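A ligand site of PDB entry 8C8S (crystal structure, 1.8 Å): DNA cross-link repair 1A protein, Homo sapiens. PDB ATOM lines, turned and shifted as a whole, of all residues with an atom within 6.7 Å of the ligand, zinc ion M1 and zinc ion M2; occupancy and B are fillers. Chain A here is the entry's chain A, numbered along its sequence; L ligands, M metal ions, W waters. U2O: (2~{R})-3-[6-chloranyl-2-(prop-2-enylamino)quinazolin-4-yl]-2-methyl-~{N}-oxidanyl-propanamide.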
ATOM      1  N   HIS A  35      12.089 -25.189  -1.524  1.00  0.00           N
ATOM      2  CA  HIS A  35      12.507 -23.874  -1.031  1.00  0.00           C
ATOM      3  C   HIS A  35      11.414 -23.256  -0.187  1.00  0.00           C
ATOM      4  O   HIS A  35      10.264 -23.687  -0.197  1.00  0.00           O
ATOM      5  CB  HIS A  35      12.884 -22.923  -2.165  1.00  0.00           C
ATOM      6  CG  HIS A  35      11.759 -22.604  -3.097  1.00  0.00           C
ATOM      7  ND1 HIS A  35      11.208 -23.543  -3.945  1.00  0.00           N
ATOM      8  CD2 HIS A  35      11.096 -21.452  -3.325  1.00  0.00           C
ATOM      9  CE1 HIS A  35      10.256 -22.967  -4.667  1.00  0.00           C
ATOM     10  NE2 HIS A  35      10.169 -21.699  -4.296  1.00  0.00           N
ATOM     11  N   PHE A  36      11.781 -22.174   0.516  1.00  0.00           N
ATOM     12  CA  PHE A  36      10.895 -21.582   1.518  1.00  0.00           C
ATOM     13  C   PHE A  36      10.090 -20.417   0.915  1.00  0.00           C
ATOM     14  O   PHE A  36      10.262 -19.244   1.245  1.00  0.00           O
ATOM     15  CB  PHE A  36      11.708 -21.143   2.731  1.00  0.00           C
ATOM     16  CG  PHE A  36      10.860 -20.784   3.929  1.00  0.00           C
ATOM     17  CD1 PHE A  36      10.255 -21.770   4.684  1.00  0.00           C
ATOM     18  CD2 PHE A  36      10.700 -19.448   4.299  1.00  0.00           C
ATOM     19  CE1 PHE A  36       9.467 -21.431   5.805  1.00  0.00           C
ATOM     20  CE2 PHE A  36       9.913 -19.109   5.421  1.00  0.00           C
ATOM     21  CZ  PHE A  36       9.306 -20.098   6.166  1.00  0.00           C
ATOM     22  N   HIS A  37       9.199 -20.766  -0.008  1.00  0.00           N
ATOM     23  CA  HIS A  37       8.188 -19.838  -0.506  1.00  0.00           C
ATOM     24  C   HIS A  37       6.808 -20.407  -0.183  1.00  0.00           C
ATOM     25  O   HIS A  37       6.608 -21.626  -0.272  1.00  0.00           O
ATOM     26  CB  HIS A  37       8.315 -19.594  -2.012  1.00  0.00           C
ATOM     27  CG  HIS A  37       9.374 -18.581  -2.366  1.00  0.00           C
ATOM     28  ND1 HIS A  37       9.938 -18.505  -3.619  1.00  0.00           N
ATOM     29  CD2 HIS A  37       9.946 -17.599  -1.641  1.00  0.00           C
ATOM     30  CE1 HIS A  37      10.817 -17.530  -3.647  1.00  0.00           C
ATOM     31  NE2 HIS A  37      10.842 -16.959  -2.455  1.00  0.00           N
ATOM     32  N   SER A  38       5.866 -19.535   0.155  1.00  0.00           N
ATOM     33  CA  SER A  38       4.602 -19.980   0.749  1.00  0.00           C
ATOM     34  C   SER A  38       3.795 -20.872  -0.171  1.00  0.00           C
ATOM     35  O   SER A  38       3.103 -21.789   0.298  1.00  0.00           O
ATOM     36  CB  SER A  38       3.768 -18.783   1.200  1.00  0.00           C
ATOM     37  OG  SER A  38       3.551 -17.874   0.136  1.00  0.00           O
ATOM     38  N   ASP A  39       3.840 -20.656  -1.488  1.00  0.00           N
ATOM     39  CA  ASP A  39       3.098 -21.558  -2.362  1.00  0.00           C
ATOM     40  C   ASP A  39       3.637 -22.983  -2.346  1.00  0.00           C
ATOM     41  O   ASP A  39       2.957 -23.892  -2.846  1.00  0.00           O
ATOM     42  CB  ASP A  39       3.052 -21.016  -3.801  1.00  0.00           C
ATOM     43  CG  ASP A  39       4.362 -20.382  -4.261  1.00  0.00           C
ATOM     44  OD1 ASP A  39       5.006 -19.673  -3.449  1.00  0.00           O
ATOM     45  OD2 ASP A  39       4.752 -20.581  -5.453  1.00  0.00           O
ATOM     46  N   HIS A  40       4.822 -23.218  -1.758  1.00  0.00           N
ATOM     47  CA  HIS A  40       5.429 -24.535  -1.691  1.00  0.00           C
ATOM     48  C   HIS A  40       5.387 -25.166  -0.317  1.00  0.00           C
ATOM     49  O   HIS A  40       5.211 -26.381  -0.199  1.00  0.00           O
ATOM     50  CB  HIS A  40       6.868 -24.468  -2.180  1.00  0.00           C
ATOM     51  CG  HIS A  40       6.981 -23.991  -3.590  1.00  0.00           C
ATOM     52  ND1 HIS A  40       7.257 -24.833  -4.644  1.00  0.00           N
ATOM     53  CD2 HIS A  40       6.786 -22.764  -4.133  1.00  0.00           C
ATOM     54  CE1 HIS A  40       7.241 -24.149  -5.773  1.00  0.00           C
ATOM     55  NE2 HIS A  40       6.952 -22.894  -5.484  1.00  0.00           N
ATOM     56  N   HIS A  96      17.354 -19.795  -7.495  1.00  0.00           N
ATOM     57  CA  HIS A  96      16.061 -19.166  -7.261  1.00  0.00           C
ATOM     58  C   HIS A  96      16.217 -18.189  -6.091  1.00  0.00           C
ATOM     59  O   HIS A  96      16.906 -17.174  -6.231  1.00  0.00           O
ATOM     60  CB  HIS A  96      15.004 -20.243  -7.004  1.00  0.00           C
ATOM     61  CG  HIS A  96      13.611 -19.739  -6.917  1.00  0.00           C
ATOM     62  ND1 HIS A  96      13.056 -18.902  -7.855  1.00  0.00           N
ATOM     63  CD2 HIS A  96      12.623 -19.998  -6.020  1.00  0.00           C
ATOM     64  CE1 HIS A  96      11.805 -18.636  -7.532  1.00  0.00           C
ATOM     65  NE2 HIS A  96      11.530 -19.283  -6.415  1.00  0.00           N
ATOM     66  N   CYS A  97      15.648 -18.489  -4.946  1.00  0.00           N
ATOM     67  CA  CYS A  97      15.869 -17.720  -3.719  1.00  0.00           C
ATOM     68  C   CYS A  97      16.878 -18.433  -2.824  1.00  0.00           C
ATOM     69  O   CYS A  97      17.263 -19.570  -3.090  1.00  0.00           O
ATOM     70  CB  CYS A  97      14.545 -17.529  -3.001  1.00  0.00           C
ATOM     71  SG  CYS A  97      13.887 -19.092  -2.436  1.00  0.00           S
ATOM     72  N   ALA A 100      17.066 -22.467  -2.124  1.00  0.00           N
ATOM     73  CA  ALA A 100      16.251 -23.171  -3.114  1.00  0.00           C
ATOM     74  C   ALA A 100      17.079 -24.234  -3.829  1.00  0.00           C
ATOM     75  O   ALA A 100      18.215 -23.976  -4.218  1.00  0.00           O
ATOM     76  CB  ALA A 100      15.677 -22.164  -4.114  1.00  0.00           C
ATOM     77  N   GLY A 117      12.180 -27.868  -8.792  1.00  0.00           N
ATOM     78  CA  GLY A 117      11.521 -26.928  -7.903  1.00  0.00           C
ATOM     79  C   GLY A 117      11.210 -25.669  -8.694  1.00  0.00           C
ATOM     80  O   GLY A 117      10.836 -25.736  -9.868  1.00  0.00           O
ATOM     81  N   ASP A 118      11.414 -24.509  -8.077  1.00  0.00           N
ATOM     82  CA  ASP A 118      11.489 -23.266  -8.836  1.00  0.00           C
ATOM     83  C   ASP A 118      12.960 -22.986  -9.154  1.00  0.00           C
ATOM     84  O   ASP A 118      13.827 -23.096  -8.282  1.00  0.00           O
ATOM     85  CB  ASP A 118      10.946 -22.081  -8.043  1.00  0.00           C
ATOM     86  CG  ASP A 118       9.424 -22.062  -7.919  1.00  0.00           C
ATOM     87  OD1 ASP A 118       8.711 -22.873  -8.540  1.00  0.00           O
ATOM     88  OD2 ASP A 118       8.984 -21.187  -7.179  1.00  0.00           O
ATOM     89  N   ASP A 141       9.877 -26.362 -13.789  1.00  0.00           N
ATOM     90  CA  ASP A 141       9.305 -25.046 -13.467  1.00  0.00           C
ATOM     91  C   ASP A 141       9.072 -24.309 -14.771  1.00  0.00           C
ATOM     92  O   ASP A 141       9.998 -23.733 -15.358  1.00  0.00           O
ATOM     93  CB  ASP A 141      10.242 -24.266 -12.541  1.00  0.00           C
ATOM     94  CG  ASP A 141       9.849 -22.787 -12.394  1.00  0.00           C
ATOM     95  OD1 ASP A 141       8.691 -22.406 -12.694  1.00  0.00           O
ATOM     96  OD2 ASP A 141      10.721 -21.996 -11.959  1.00  0.00           O
ATOM     97  N   THR A 143       7.121 -21.589 -15.246  1.00  0.00           N
ATOM     98  CA  THR A 143       6.440 -20.331 -14.933  1.00  0.00           C
ATOM     99  C   THR A 143       6.356 -19.420 -16.156  1.00  0.00           C
ATOM    100  O   THR A 143       5.289 -18.855 -16.454  1.00  0.00           O
ATOM    101  CB  THR A 143       7.172 -19.622 -13.784  1.00  0.00           C
ATOM    102  OG1 THR A 143       7.153 -20.474 -12.628  1.00  0.00           O
ATOM    103  CG2 THR A 143       6.508 -18.280 -13.404  1.00  0.00           C
ATOM    104  N   TYR A 144       7.451 -19.284 -16.891  1.00  0.00           N
ATOM    105  CA  TYR A 144       7.567 -18.391 -18.031  1.00  0.00           C
ATOM    106  C   TYR A 144       7.825 -19.161 -19.318  1.00  0.00           C
ATOM    107  O   TYR A 144       8.652 -18.764 -20.151  1.00  0.00           O
ATOM    108  CB  TYR A 144       8.668 -17.358 -17.772  1.00  0.00           C
ATOM    109  CG  TYR A 144       8.319 -16.375 -16.688  1.00  0.00           C
ATOM    110  CD1 TYR A 144       7.122 -15.684 -16.732  1.00  0.00           C
ATOM    111  CD2 TYR A 144       9.173 -16.146 -15.626  1.00  0.00           C
ATOM    112  CE1 TYR A 144       6.775 -14.775 -15.742  1.00  0.00           C
ATOM    113  CE2 TYR A 144       8.847 -15.235 -14.629  1.00  0.00           C
ATOM    114  CZ  TYR A 144       7.646 -14.554 -14.701  1.00  0.00           C
ATOM    115  OH  TYR A 144       7.295 -13.669 -13.723  1.00  0.00           O
ATOM    116  N   TYR A 182       8.328  -9.190  -0.221  1.00  0.00           N
ATOM    117  CA  TYR A 182       7.155  -9.998   0.095  1.00  0.00           C
ATOM    118  C   TYR A 182       7.500 -11.333   0.725  1.00  0.00           C
ATOM    119  O   TYR A 182       6.663 -11.891   1.451  1.00  0.00           O
ATOM    120  CB  TYR A 182       6.316 -10.244  -1.176  1.00  0.00           C
ATOM    121  N   SER A 183       8.681 -11.856   0.474  1.00  0.00           N
ATOM    122  CA  SER A 183       9.122 -13.166   0.944  1.00  0.00           C
ATOM    123  C   SER A 183      10.627 -13.214   0.694  1.00  0.00           C
ATOM    124  O   SER A 183      11.238 -12.207   0.324  1.00  0.00           O
ATOM    125  CB  SER A 183       8.374 -14.306   0.242  1.00  0.00           C
ATOM    126  OG  SER A 183       8.534 -14.251  -1.156  1.00  0.00           O
ATOM    127  N   ILE A 184      11.247 -14.368   0.908  1.00  0.00           N
ATOM    128  CA  ILE A 184      12.681 -14.421   0.660  1.00  0.00           C
ATOM    129  C   ILE A 184      12.933 -14.420  -0.852  1.00  0.00           C
ATOM    130  O   ILE A 184      12.035 -14.660  -1.670  1.00  0.00           O
ATOM    131  CB  ILE A 184      13.357 -15.630   1.328  1.00  0.00           C
ATOM    132  CG1 ILE A 184      12.829 -16.943   0.755  1.00  0.00           C
ATOM    133  CG2 ILE A 184      13.185 -15.566   2.860  1.00  0.00           C
ATOM    134  CD1 ILE A 184      13.689 -18.145   1.161  1.00  0.00           C
ATOM    135  N   LYS A 186      15.564 -12.236  -3.954  1.00  0.00           N
ATOM    136  CA  LYS A 186      15.775 -10.900  -4.497  1.00  0.00           C
ATOM    137  C   LYS A 186      16.472  -9.977  -3.507  1.00  0.00           C
ATOM    138  O   LYS A 186      16.413  -8.762  -3.643  1.00  0.00           O
ATOM    139  CB  LYS A 186      14.439 -10.299  -4.969  1.00  0.00           C
ATOM    140  CG  LYS A 186      13.626 -11.270  -5.874  1.00  0.00           C
ATOM    141  CD  LYS A 186      12.430 -10.605  -6.599  1.00  0.00           C
ATOM    142  CE  LYS A 186      11.623 -11.634  -7.391  1.00  0.00           C
ATOM    143  NZ  LYS A 186      10.538 -10.973  -8.205  1.00  0.00           N
ATOM    144  N   GLY A 266       8.203  -9.582 -11.157  1.00  0.00           N
ATOM    145  CA  GLY A 266       8.646 -10.534 -12.158  1.00  0.00           C
ATOM    146  C   GLY A 266       8.513  -9.923 -13.532  1.00  0.00           C
ATOM    147  O   GLY A 266       8.759  -8.727 -13.728  1.00  0.00           O
ATOM    148  N   TRP A 267       8.123 -10.735 -14.508  1.00  0.00           N
ATOM    149  CA  TRP A 267       7.813 -10.226 -15.844  1.00  0.00           C
ATOM    150  C   TRP A 267       6.587  -9.326 -15.802  1.00  0.00           C
ATOM    151  O   TRP A 267       5.631  -9.588 -15.068  1.00  0.00           O
ATOM    152  CB  TRP A 267       7.579 -11.392 -16.805  1.00  0.00           C
ATOM    153  CG  TRP A 267       7.083 -10.975 -18.169  1.00  0.00           C
ATOM    154  CD1 TRP A 267       7.854 -10.657 -19.254  1.00  0.00           C
ATOM    155  CD2 TRP A 267       5.725 -10.839 -18.584  1.00  0.00           C
ATOM    156  NE1 TRP A 267       7.050 -10.319 -20.314  1.00  0.00           N
ATOM    157  CE2 TRP A 267       5.735 -10.431 -19.935  1.00  0.00           C
ATOM    158  CE3 TRP A 267       4.492 -11.021 -17.951  1.00  0.00           C
ATOM    159  CZ2 TRP A 267       4.564 -10.200 -20.662  1.00  0.00           C
ATOM    160  CZ3 TRP A 267       3.320 -10.800 -18.675  1.00  0.00           C
ATOM    161  CH2 TRP A 267       3.371 -10.393 -20.022  1.00  0.00           C
ATOM    162  N   GLU A 296      13.597 -14.405 -10.487  1.00  0.00           N
ATOM    163  CA  GLU A 296      14.253 -15.611 -10.007  1.00  0.00           C
ATOM    164  C   GLU A 296      13.645 -16.852 -10.633  1.00  0.00           C
ATOM    165  O   GLU A 296      13.817 -17.972 -10.121  1.00  0.00           O
ATOM    166  CB  GLU A 296      14.220 -15.661  -8.470  1.00  0.00           C
ATOM    167  CG  GLU A 296      15.105 -14.519  -7.895  1.00  0.00           C
ATOM    168  CD  GLU A 296      15.344 -14.572  -6.376  1.00  0.00           C
ATOM    169  OE1 GLU A 296      14.473 -15.082  -5.639  1.00  0.00           O
ATOM    170  OE2 GLU A 296      16.417 -14.089  -5.937  1.00  0.00           O
ATOM    171  N   HIS A 297      12.939 -16.677 -11.751  1.00  0.00           N
ATOM    172  CA  HIS A 297      12.522 -17.760 -12.626  1.00  0.00           C
ATOM    173  C   HIS A 297      13.160 -17.612 -13.998  1.00  0.00           C
ATOM    174  O   HIS A 297      13.407 -16.490 -14.478  1.00  0.00           O
ATOM    175  CB  HIS A 297      10.980 -17.786 -12.803  1.00  0.00           C
ATOM    176  CG  HIS A 297      10.213 -18.149 -11.566  1.00  0.00           C
ATOM    177  ND1 HIS A 297       9.997 -19.453 -11.181  1.00  0.00           N
ATOM    178  CD2 HIS A 297       9.580 -17.371 -10.651  1.00  0.00           C
ATOM    179  CE1 HIS A 297       9.281 -19.471 -10.073  1.00  0.00           C
ATOM    180  NE2 HIS A 297       9.008 -18.221  -9.732  1.00  0.00           N
ATOM    181  N   VAL A 319       4.009 -25.834 -13.375  1.00  0.00           N
ATOM    182  CA  VAL A 319       3.410 -24.502 -13.299  1.00  0.00           C
ATOM    183  C   VAL A 319       2.581 -24.281 -14.562  1.00  0.00           C
ATOM    184  O   VAL A 319       2.912 -24.776 -15.640  1.00  0.00           O
ATOM    185  CB  VAL A 319       4.496 -23.390 -13.158  1.00  0.00           C
ATOM    186  CG1 VAL A 319       3.843 -22.001 -12.986  1.00  0.00           C
ATOM    187  CG2 VAL A 319       5.448 -23.674 -11.999  1.00  0.00           C
HETATM  188  C1  U2O L   1       8.369 -15.280  -4.757  1.00  0.00           C
HETATM  189  C10 U2O L   1       2.632 -17.279  -6.344  1.00  0.00           C
HETATM  190  C11 U2O L   1       4.216 -16.878  -8.000  1.00  0.00           C
HETATM  191  C12 U2O L   1       5.830 -16.424  -9.805  1.00  0.00           C
HETATM  192  C13 U2O L   1       5.750 -15.389 -10.845  1.00  0.00           C
HETATM  193  C14 U2O L   1       4.666 -14.914 -11.388  1.00  0.00           C
HETATM  194  C15 U2O L   1       7.865 -17.534  -5.743  1.00  0.00           C
HETATM  195  C2  U2O L   1       7.351 -16.106  -5.551  1.00  0.00           C
HETATM  196  C3  U2O L   1       5.972 -16.110  -4.858  1.00  0.00           C
HETATM  197  C4  U2O L   1       4.879 -16.517  -5.807  1.00  0.00           C
HETATM  198  C5  U2O L   1       3.573 -16.913  -5.360  1.00  0.00           C
HETATM  199  C6  U2O L   1       3.199 -16.936  -4.003  1.00  0.00           C
HETATM  200  C7  U2O L   1       1.932 -17.317  -3.662  1.00  0.00           C
HETATM  201  C8  U2O L   1       0.982 -17.688  -4.633  1.00  0.00           C
HETATM  202  C9  U2O L   1       1.330 -17.672  -5.951  1.00  0.00           C
HETATM  203  N1  U2O L   1       2.969 -17.255  -7.674  1.00  0.00           N
HETATM  204  N2  U2O L   1       4.535 -16.865  -9.302  1.00  0.00           N
HETATM  205  N3  U2O L   1       5.177 -16.505  -7.116  1.00  0.00           N
HETATM  206  N4  U2O L   1       7.197 -18.488  -5.127  1.00  0.00           N
HETATM  207  O1  U2O L   1       7.575 -19.819  -5.277  1.00  0.00           O
HETATM  208  O2  U2O L   1       8.831 -17.766  -6.469  1.00  0.00           O
HETATM  209 CL1  U2O L   1       1.461 -17.355  -1.990  1.00  0.00          CL
HETATM  210 ZN    ZN M   1       9.615 -19.797  -5.427  1.00  0.00          ZN
HETATM  211 ZN    ZN M   2       6.835 -21.038  -6.728  1.00  0.00          ZN
HETATM  212  O   HOH W   1       6.372 -22.233  -8.526  1.00  0.00           O
HETATM  213  O   HOH W   2       6.771 -19.160  -7.797  1.00  0.00           O
HETATM  214  O   HOH W   3      10.022 -15.562  -7.573  1.00  0.00           O
HETATM  215  O   HOH W   4       5.916 -16.602  -1.692  1.00  0.00           O
HETATM  216  O   HOH W   5       5.611 -20.006 -10.345  1.00  0.00           O
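The nearest printed residue that does not touch zinc ion M1 is His 40 (4.1 Å).
Zinc ion M1 is bound by an oxygen (O1) of the ligand (2.0 Å), a ring nitrogen (NE2) of His 96 (2.2 Å), a ring nitrogen (ND1) of His 37 (2.2 Å), a ring nitrogen (NE2) of His 35 (2.3 Å), the side-chain carboxylate (OD2) of Asp 118 (2.3 Å) and an oxygen (O2) of the ligand (2.4 Å).
The nearest printed residue that does not touch zinc ion M2 is His 35 (4.2 Å).
Merely in contact with the ligand: Ser 38 (3.0 Å), Thr 143 (3.9 Å), Tyr 144 (3.7 Å) and Ser 183 (3.7 Å).
Hydrophobic or aromatic side chains that line the ligand: His 37, His 40, His 96 and His 297.
Of the 23 residues printed, 11 come within 4 Å of the ligand.
The nearest printed residue that does not touch the ligand is Ile 184 (4.8 Å).
A ring nitrogen (ND1) of His 96 lies within hydrogen-bond range of the backbone carbonyl oxygen (O) of Glu 296, at 2.6 Å.
The backbone carbonyl oxygen (O) of Ile 184 sits at hydrogen-bond distance from a ring nitrogen (NE2) of His 37 (2.7 Å).
The side-chain sulfur (SG) of Cys 97 sits close to a ring nitrogen (NE2) of His 37, at 3.7 Å.
The side-chain hydroxyl (OG1) of Thr 143 is in hydrogen-bond range of a ring nitrogen (ND1) of His 297.
The side-chain carboxylate of Asp 141 is in hydrogen-bond range of a ring nitrogen (ND1) of His 297, at 2.8 Å.
The backbone NH (N) of Trp 267 lies within hydrogen-bond range of the side-chain hydroxyl (OH) of Tyr 144 (3.1 Å).
OD1 of Asp 141 lies within hydrogen-bond range of OG1 of Thr 143 (2.5 Å).
O1 of the ligand binds zinc ion M2.
Zinc ion M2 is bound by water W2.
Zinc ion M2 is bound by OD2 of Asp 118 (2.2 Å).
Water W1 is bound to zinc ion M2, at 2.2 Å.
NE2 of His 40 is bound to zinc ion M2 (2.2 Å).
OD2 of Asp 39 binds zinc ion M2 (2.5 Å).
Zinc ion M2 has six donor atoms within binding distance.
Water W2 lies within hydrogen-bond range of a nitrogen (N4) of the ligand (2.8 Å) and a ring nitrogen (NE2) of His 297 (3.1 Å).
Water W5 bridges the side-chain hydroxyl of Thr 143 (2.8 Å) and a nitrogen (N2) of the ligand (3.5 Å).
A ring nitrogen (NE2) of His 297 sits close to an oxygen (O2) of the ligand, at 3.3 Å.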
